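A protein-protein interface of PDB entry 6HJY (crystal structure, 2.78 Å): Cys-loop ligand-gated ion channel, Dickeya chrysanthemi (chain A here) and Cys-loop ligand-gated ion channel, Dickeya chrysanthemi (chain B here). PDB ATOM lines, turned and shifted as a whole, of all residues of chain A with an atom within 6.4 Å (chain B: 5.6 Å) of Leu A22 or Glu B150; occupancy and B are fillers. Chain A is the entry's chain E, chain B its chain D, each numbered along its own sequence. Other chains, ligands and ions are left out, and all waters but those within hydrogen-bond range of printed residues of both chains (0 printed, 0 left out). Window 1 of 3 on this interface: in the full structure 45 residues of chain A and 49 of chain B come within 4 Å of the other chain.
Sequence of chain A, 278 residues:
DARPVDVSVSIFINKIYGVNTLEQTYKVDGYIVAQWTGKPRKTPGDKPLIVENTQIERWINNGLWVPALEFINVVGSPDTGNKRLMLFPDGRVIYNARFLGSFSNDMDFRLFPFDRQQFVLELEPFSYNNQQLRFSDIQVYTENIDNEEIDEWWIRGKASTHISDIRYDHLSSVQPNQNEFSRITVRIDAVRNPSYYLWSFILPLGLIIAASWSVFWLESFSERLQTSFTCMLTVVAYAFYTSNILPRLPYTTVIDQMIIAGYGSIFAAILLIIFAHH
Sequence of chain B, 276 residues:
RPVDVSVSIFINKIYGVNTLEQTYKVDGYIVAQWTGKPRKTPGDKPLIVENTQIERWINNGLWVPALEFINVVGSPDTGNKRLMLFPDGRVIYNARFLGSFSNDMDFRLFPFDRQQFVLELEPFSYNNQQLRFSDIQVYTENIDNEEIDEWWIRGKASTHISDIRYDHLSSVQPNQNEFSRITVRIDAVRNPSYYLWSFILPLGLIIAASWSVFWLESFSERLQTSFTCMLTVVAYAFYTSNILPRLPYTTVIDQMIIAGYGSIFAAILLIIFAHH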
ATOM      1  N   ASN A  20      29.056 -22.103  27.573  1.00  0.00           N
ATOM      2  CA  ASN A  20      27.866 -22.801  27.109  1.00  0.00           C
ATOM      3  C   ASN A  20      27.893 -22.666  25.590  1.00  0.00           C
ATOM      4  O   ASN A  20      27.581 -21.602  25.049  1.00  0.00           O
ATOM      5  CB  ASN A  20      26.581 -22.217  27.716  1.00  0.00           C
ATOM      6  CG  ASN A  20      25.319 -22.991  27.381  1.00  0.00           C
ATOM      7  OD1 ASN A  20      25.071 -23.397  26.239  1.00  0.00           O
ATOM      8  ND2 ASN A  20      24.462 -23.165  28.367  1.00  0.00           N
ATOM      9  N   THR A  21      28.328 -23.746  24.921  1.00  0.00           N
ATOM     10  CA  THR A  21      28.481 -23.862  23.468  1.00  0.00           C
ATOM     11  C   THR A  21      27.215 -23.519  22.667  1.00  0.00           C
ATOM     12  O   THR A  21      27.299 -22.755  21.703  1.00  0.00           O
ATOM     13  CB  THR A  21      29.003 -25.257  23.081  1.00  0.00           C
ATOM     14  OG1 THR A  21      28.163 -26.251  23.670  1.00  0.00           O
ATOM     15  CG2 THR A  21      30.455 -25.477  23.475  1.00  0.00           C
ATOM     16  N   LEU A  22      26.052 -24.079  23.060  1.00  0.00           N
ATOM     17  CA  LEU A  22      24.795 -23.848  22.346  1.00  0.00           C
ATOM     18  C   LEU A  22      24.232 -22.442  22.550  1.00  0.00           C
ATOM     19  O   LEU A  22      23.689 -21.862  21.609  1.00  0.00           O
ATOM     20  CB  LEU A  22      23.753 -24.926  22.681  1.00  0.00           C
ATOM     21  CG  LEU A  22      22.660 -25.179  21.628  1.00  0.00           C
ATOM     22  CD1 LEU A  22      23.237 -25.393  20.226  1.00  0.00           C
ATOM     23  CD2 LEU A  22      21.794 -26.349  22.021  1.00  0.00           C
ATOM     24  N   GLU A  23      24.386 -21.884  23.759  1.00  0.00           N
ATOM     25  CA  GLU A  23      23.925 -20.533  24.067  1.00  0.00           C
ATOM     26  C   GLU A  23      24.933 -19.461  23.640  1.00  0.00           C
ATOM     27  O   GLU A  23      24.582 -18.277  23.626  1.00  0.00           O
ATOM     28  CB  GLU A  23      23.629 -20.388  25.565  1.00  0.00           C
ATOM     29  CG  GLU A  23      22.351 -21.073  26.014  1.00  0.00           C
ATOM     30  CD  GLU A  23      21.868 -20.711  27.410  1.00  0.00           C
ATOM     31  OE1 GLU A  23      22.614 -20.037  28.160  1.00  0.00           O
ATOM     32  OE2 GLU A  23      20.742 -21.126  27.764  1.00  0.00           O
ATOM     33  N   GLN A  24      26.187 -19.869  23.317  1.00  0.00           N
ATOM     34  CA  GLN A  24      27.304 -18.990  22.945  1.00  0.00           C
ATOM     35  C   GLN A  24      27.562 -17.937  24.028  1.00  0.00           C
ATOM     36  O   GLN A  24      27.710 -16.750  23.735  1.00  0.00           O
ATOM     37  CB  GLN A  24      27.132 -18.380  21.544  1.00  0.00           C
ATOM     38  CG  GLN A  24      27.570 -19.295  20.416  1.00  0.00           C
ATOM     39  CD  GLN A  24      27.262 -18.664  19.092  1.00  0.00           C
ATOM     40  OE1 GLN A  24      28.007 -17.829  18.587  1.00  0.00           O
ATOM     41  NE2 GLN A  24      26.123 -19.008  18.526  1.00  0.00           N
ATOM     42  N   THR A  25      27.608 -18.406  25.293  1.00  0.00           N
ATOM     43  CA  THR A  25      27.856 -17.610  26.496  1.00  0.00           C
ATOM     44  C   THR A  25      29.028 -18.189  27.305  1.00  0.00           C
ATOM     45  O   THR A  25      29.426 -19.337  27.098  1.00  0.00           O
ATOM     46  CB  THR A  25      26.579 -17.460  27.360  1.00  0.00           C
ATOM     47  OG1 THR A  25      26.095 -18.741  27.765  1.00  0.00           O
ATOM     48  CG2 THR A  25      25.480 -16.658  26.675  1.00  0.00           C
ATOM     49  N   PHE A 109      32.706 -23.274  17.188  1.00  0.00           N
ATOM     50  CA  PHE A 109      33.267 -24.508  17.735  1.00  0.00           C
ATOM     51  C   PHE A 109      33.467 -25.609  16.674  1.00  0.00           C
ATOM     52  O   PHE A 109      33.641 -26.773  17.040  1.00  0.00           O
ATOM     53  CB  PHE A 109      32.388 -25.018  18.897  1.00  0.00           C
ATOM     54  CG  PHE A 109      32.128 -24.032  20.014  1.00  0.00           C
ATOM     55  CD1 PHE A 109      33.041 -23.872  21.049  1.00  0.00           C
ATOM     56  CD2 PHE A 109      30.951 -23.297  20.054  1.00  0.00           C
ATOM     57  CE1 PHE A 109      32.793 -22.972  22.089  1.00  0.00           C
ATOM     58  CE2 PHE A 109      30.699 -22.412  21.098  1.00  0.00           C
ATOM     59  CZ  PHE A 109      31.618 -22.259  22.111  1.00  0.00           C
ATOM     60  N   PRO A 247      29.957 -31.382  23.691  1.00  0.00           N
ATOM     61  CA  PRO A 247      28.979 -30.303  23.882  1.00  0.00           C
ATOM     62  C   PRO A 247      27.915 -30.235  22.789  1.00  0.00           C
ATOM     63  O   PRO A 247      28.179 -30.611  21.642  1.00  0.00           O
ATOM     64  CB  PRO A 247      29.852 -29.049  23.895  1.00  0.00           C
ATOM     65  CG  PRO A 247      31.037 -29.402  23.076  1.00  0.00           C
ATOM     66  CD  PRO A 247      31.300 -30.840  23.384  1.00  0.00           C
ATOM     67  N   ARG A 248      26.711 -29.737  23.153  1.00  0.00           N
ATOM     68  CA  ARG A 248      25.592 -29.577  22.225  1.00  0.00           C
ATOM     69  C   ARG A 248      25.867 -28.464  21.224  1.00  0.00           C
ATOM     70  O   ARG A 248      26.149 -27.333  21.620  1.00  0.00           O
ATOM     71  CB  ARG A 248      24.254 -29.360  22.959  1.00  0.00           C
ATOM     72  CG  ARG A 248      23.617 -30.646  23.517  1.00  0.00           C
ATOM     73  CD  ARG A 248      23.351 -31.755  22.486  1.00  0.00           C
ATOM     74  NE  ARG A 248      22.629 -31.276  21.302  1.00  0.00           N
ATOM     75  CZ  ARG A 248      23.119 -31.271  20.063  1.00  0.00           C
ATOM     76  NH1 ARG A 248      24.339 -31.732  19.820  1.00  0.00           N
ATOM     77  NH2 ARG A 248      22.382 -30.821  19.056  1.00  0.00           N
ATOM     78  N   LEU A 249      25.854 -28.812  19.925  1.00  0.00           N
ATOM     79  CA  LEU A 249      26.142 -27.881  18.836  1.00  0.00           C
ATOM     80  C   LEU A 249      25.206 -28.058  17.628  1.00  0.00           C
ATOM     81  O   LEU A 249      24.748 -29.175  17.358  1.00  0.00           O
ATOM     82  CB  LEU A 249      27.617 -28.021  18.399  1.00  0.00           C
ATOM     83  CG  LEU A 249      28.677 -27.469  19.354  1.00  0.00           C
ATOM     84  CD1 LEU A 249      30.027 -28.011  19.015  1.00  0.00           C
ATOM     85  CD2 LEU A 249      28.706 -25.951  19.334  1.00  0.00           C
ATOM     86  N   PRO A 250      24.933 -26.971  16.862  1.00  0.00           N
ATOM     87  CA  PRO A 250      24.059 -27.113  15.687  1.00  0.00           C
ATOM     88  C   PRO A 250      24.794 -27.555  14.411  1.00  0.00           C
ATOM     89  O   PRO A 250      24.180 -27.601  13.347  1.00  0.00           O
ATOM     90  CB  PRO A 250      23.478 -25.711  15.539  1.00  0.00           C
ATOM     91  CG  PRO A 250      24.560 -24.808  16.026  1.00  0.00           C
ATOM     92  CD  PRO A 250      25.384 -25.572  17.027  1.00  0.00           C
ATOM     93  N   GLU B 146      25.542 -17.094   9.915  1.00  0.00           N
ATOM     94  CA  GLU B 146      24.512 -17.933  10.533  1.00  0.00           C
ATOM     95  C   GLU B 146      24.903 -19.414  10.618  1.00  0.00           C
ATOM     96  O   GLU B 146      24.224 -20.182  11.304  1.00  0.00           O
ATOM     97  CB  GLU B 146      23.152 -17.749   9.828  1.00  0.00           C
ATOM     98  CG  GLU B 146      23.138 -18.119   8.349  1.00  0.00           C
ATOM     99  CD  GLU B 146      21.771 -18.276   7.701  1.00  0.00           C
ATOM    100  OE1 GLU B 146      20.827 -17.548   8.079  1.00  0.00           O
ATOM    101  OE2 GLU B 146      21.653 -19.113   6.776  1.00  0.00           O
ATOM    102  N   ILE B 148      27.375 -20.728  12.179  1.00  0.00           N
ATOM    103  CA  ILE B 148      27.740 -20.963  13.574  1.00  0.00           C
ATOM    104  C   ILE B 148      26.526 -20.870  14.540  1.00  0.00           C
ATOM    105  O   ILE B 148      26.679 -21.152  15.732  1.00  0.00           O
ATOM    106  CB  ILE B 148      28.936 -20.049  14.004  1.00  0.00           C
ATOM    107  CG1 ILE B 148      28.517 -18.577  14.235  1.00  0.00           C
ATOM    108  CG2 ILE B 148      30.103 -20.157  13.002  1.00  0.00           C
ATOM    109  CD1 ILE B 148      29.273 -17.854  15.363  1.00  0.00           C
ATOM    110  N   ASP B 149      25.331 -20.482  14.024  1.00  0.00           N
ATOM    111  CA  ASP B 149      24.092 -20.321  14.801  1.00  0.00           C
ATOM    112  C   ASP B 149      23.108 -21.496  14.668  1.00  0.00           C
ATOM    113  O   ASP B 149      22.967 -22.073  13.589  1.00  0.00           O
ATOM    114  CB  ASP B 149      23.381 -19.009  14.417  1.00  0.00           C
ATOM    115  CG  ASP B 149      24.172 -17.742  14.673  1.00  0.00           C
ATOM    116  OD1 ASP B 149      24.818 -17.649  15.737  1.00  0.00           O
ATOM    117  OD2 ASP B 149      24.095 -16.821  13.841  1.00  0.00           O
ATOM    118  N   GLU B 150      22.389 -21.796  15.769  1.00  0.00           N
ATOM    119  CA  GLU B 150      21.382 -22.856  15.880  1.00  0.00           C
ATOM    120  C   GLU B 150      20.116 -22.539  15.084  1.00  0.00           C
ATOM    121  O   GLU B 150      19.521 -23.444  14.489  1.00  0.00           O
ATOM    122  CB  GLU B 150      21.046 -23.119  17.359  1.00  0.00           C
ATOM    123  CG  GLU B 150      20.229 -24.381  17.609  1.00  0.00           C
ATOM    124  CD  GLU B 150      19.773 -24.622  19.042  1.00  0.00           C
ATOM    125  OE1 GLU B 150      20.098 -23.800  19.930  1.00  0.00           O
ATOM    126  OE2 GLU B 150      19.063 -25.627  19.272  1.00  0.00           O
ATOM    127  N   TRP B 151      19.701 -21.258  15.099  1.00  0.00           N
ATOM    128  CA  TRP B 151      18.532 -20.747  14.392  1.00  0.00           C
ATOM    129  C   TRP B 151      18.928 -19.777  13.294  1.00  0.00           C
ATOM    130  O   TRP B 151      19.910 -19.038  13.429  1.00  0.00           O
ATOM    131  CB  TRP B 151      17.550 -20.091  15.366  1.00  0.00           C
ATOM    132  CG  TRP B 151      16.885 -21.092  16.258  1.00  0.00           C
ATOM    133  CD1 TRP B 151      17.247 -21.427  17.530  1.00  0.00           C
ATOM    134  CD2 TRP B 151      15.798 -21.960  15.907  1.00  0.00           C
ATOM    135  NE1 TRP B 151      16.429 -22.427  18.009  1.00  0.00           N
ATOM    136  CE2 TRP B 151      15.536 -22.779  17.029  1.00  0.00           C
ATOM    137  CE3 TRP B 151      15.006 -22.109  14.759  1.00  0.00           C
ATOM    138  CZ2 TRP B 151      14.518 -23.743  17.028  1.00  0.00           C
ATOM    139  CZ3 TRP B 151      14.001 -23.063  14.759  1.00  0.00           C
ATOM    140  CH2 TRP B 151      13.773 -23.877  15.876  1.00  0.00           C
ATOM    141  N   TRP B 152      18.162 -19.798  12.194  1.00  0.00           N
ATOM    142  CA  TRP B 152      18.375 -18.942  11.036  1.00  0.00           C
ATOM    143  C   TRP B 152      17.184 -18.019  10.847  1.00  0.00           C
ATOM    144  O   TRP B 152      16.129 -18.452  10.383  1.00  0.00           O
ATOM    145  CB  TRP B 152      18.635 -19.779   9.772  1.00  0.00           C
ATOM    146  CG  TRP B 152      19.891 -20.612   9.786  1.00  0.00           C
ATOM    147  CD1 TRP B 152      20.990 -20.443  10.577  1.00  0.00           C
ATOM    148  CD2 TRP B 152      20.187 -21.710   8.914  1.00  0.00           C
ATOM    149  NE1 TRP B 152      21.937 -21.400  10.286  1.00  0.00           N
ATOM    150  CE2 TRP B 152      21.479 -22.178   9.252  1.00  0.00           C
ATOM    151  CE3 TRP B 152      19.485 -22.348   7.876  1.00  0.00           C
ATOM    152  CZ2 TRP B 152      22.086 -23.247   8.575  1.00  0.00           C
ATOM    153  CZ3 TRP B 152      20.078 -23.417   7.225  1.00  0.00           C
ATOM    154  CH2 TRP B 152      21.356 -23.868   7.585  1.00  0.00           C
ATOM    155  N   VAL B 189      14.330 -20.559  11.022  1.00  0.00           N
ATOM    156  CA  VAL B 189      14.469 -21.937  10.524  1.00  0.00           C
ATOM    157  C   VAL B 189      15.572 -22.597  11.365  1.00  0.00           C
ATOM    158  O   VAL B 189      16.544 -21.925  11.725  1.00  0.00           O
ATOM    159  CB  VAL B 189      14.862 -21.949   9.014  1.00  0.00           C
ATOM    160  CG1 VAL B 189      15.046 -23.371   8.487  1.00  0.00           C
ATOM    161  CG2 VAL B 189      13.830 -21.220   8.165  1.00  0.00           C
ATOM    162  N   ARG B 190      15.428 -23.893  11.693  1.00  0.00           N
ATOM    163  CA  ARG B 190      16.484 -24.577  12.433  1.00  0.00           C
ATOM    164  C   ARG B 190      17.628 -24.918  11.484  1.00  0.00           C
ATOM    165  O   ARG B 190      17.387 -25.215  10.314  1.00  0.00           O
ATOM    166  CB  ARG B 190      15.966 -25.856  13.101  1.00  0.00           C
ATOM    167  CG  ARG B 190      16.920 -26.378  14.178  1.00  0.00           C
ATOM    168  CD  ARG B 190      16.482 -27.702  14.759  1.00  0.00           C
ATOM    169  NE  ARG B 190      15.181 -27.589  15.421  1.00  0.00           N
ATOM    170  CZ  ARG B 190      14.995 -27.249  16.693  1.00  0.00           C
ATOM    171  NH1 ARG B 190      16.033 -26.993  17.481  1.00  0.00           N
ATOM    172  NH2 ARG B 190      13.769 -27.167  17.190  1.00  0.00           N
ATOM    173  N   ASN B 191      18.874 -24.839  11.989  1.00  0.00           N
ATOM    174  CA  ASN B 191      20.090 -25.218  11.275  1.00  0.00           C
ATOM    175  C   ASN B 191      20.125 -26.763  11.369  1.00  0.00           C
ATOM    176  O   ASN B 191      20.324 -27.292  12.470  1.00  0.00           O
ATOM    177  CB  ASN B 191      21.322 -24.581  11.970  1.00  0.00           C
ATOM    178  CG  ASN B 191      22.686 -24.876  11.373  1.00  0.00           C
ATOM    179  OD1 ASN B 191      22.874 -25.773  10.546  1.00  0.00           O
ATOM    180  ND2 ASN B 191      23.674 -24.087  11.759  1.00  0.00           N
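The side-chain carboxylate of Asp B149 lies within hydrogen-bond range of the side-chain amide nitrogen of Gln A24 (3.4 Å).
Hydrophobic or aromatic side chains of chain A within 4 Å of the printed part of chain B: Leu A22 and Pro A250. Printed residues of chain B that touch a printed residue of chain A: Ile B148, Asp B149, Glu B150 and Asn B191. Hydrophobic or aromatic side chains of chain B within 4 Å of the printed part of chain A: Ile B148.
Leu A22 touches Glu B150. Gln A24 touches Ile B148. Asp B149 touches Pro A250. Pro A250 touches Glu B150. Asn B191 touches Pro A250.
Glu B150 touches just these residues of chain A: Leu A22 and Pro A250. Of the printed residues of chain A, Ile B148 touches Gln A24 (3.5 Å). Of the printed residues of chain B, Gln A24 touches Ile B148 and Asp B149. Of the printed residues of chain B, Pro A250 touches Asp B149, Glu B150 and Asn B191. Of the printed residues of chain A, Asn B191 touches Pro A250 (3.6 Å). Leu A249 touches none of the printed residues of chain B.
The backbone carbonyl oxygen (O) of Asp B149 is in hydrogen-bond range of the side-chain amide nitrogen (ND2) of Asn B191, at 2.8 Å. The side-chain carboxylate (OE2) of Glu B150 lies within salt-bridge range of the guanidinium group (NH1) of Arg B190 (3.8 Å). The backbone carbonyl oxygen of Glu B150 lies within hydrogen-bond range of the backbone NH of Asn B191 (2.9 Å). The side-chain amide oxygen (OD1) of Asn A20 lies within hydrogen-bond range of the backbone NH (N) of Leu A22, at 3.4 Å.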
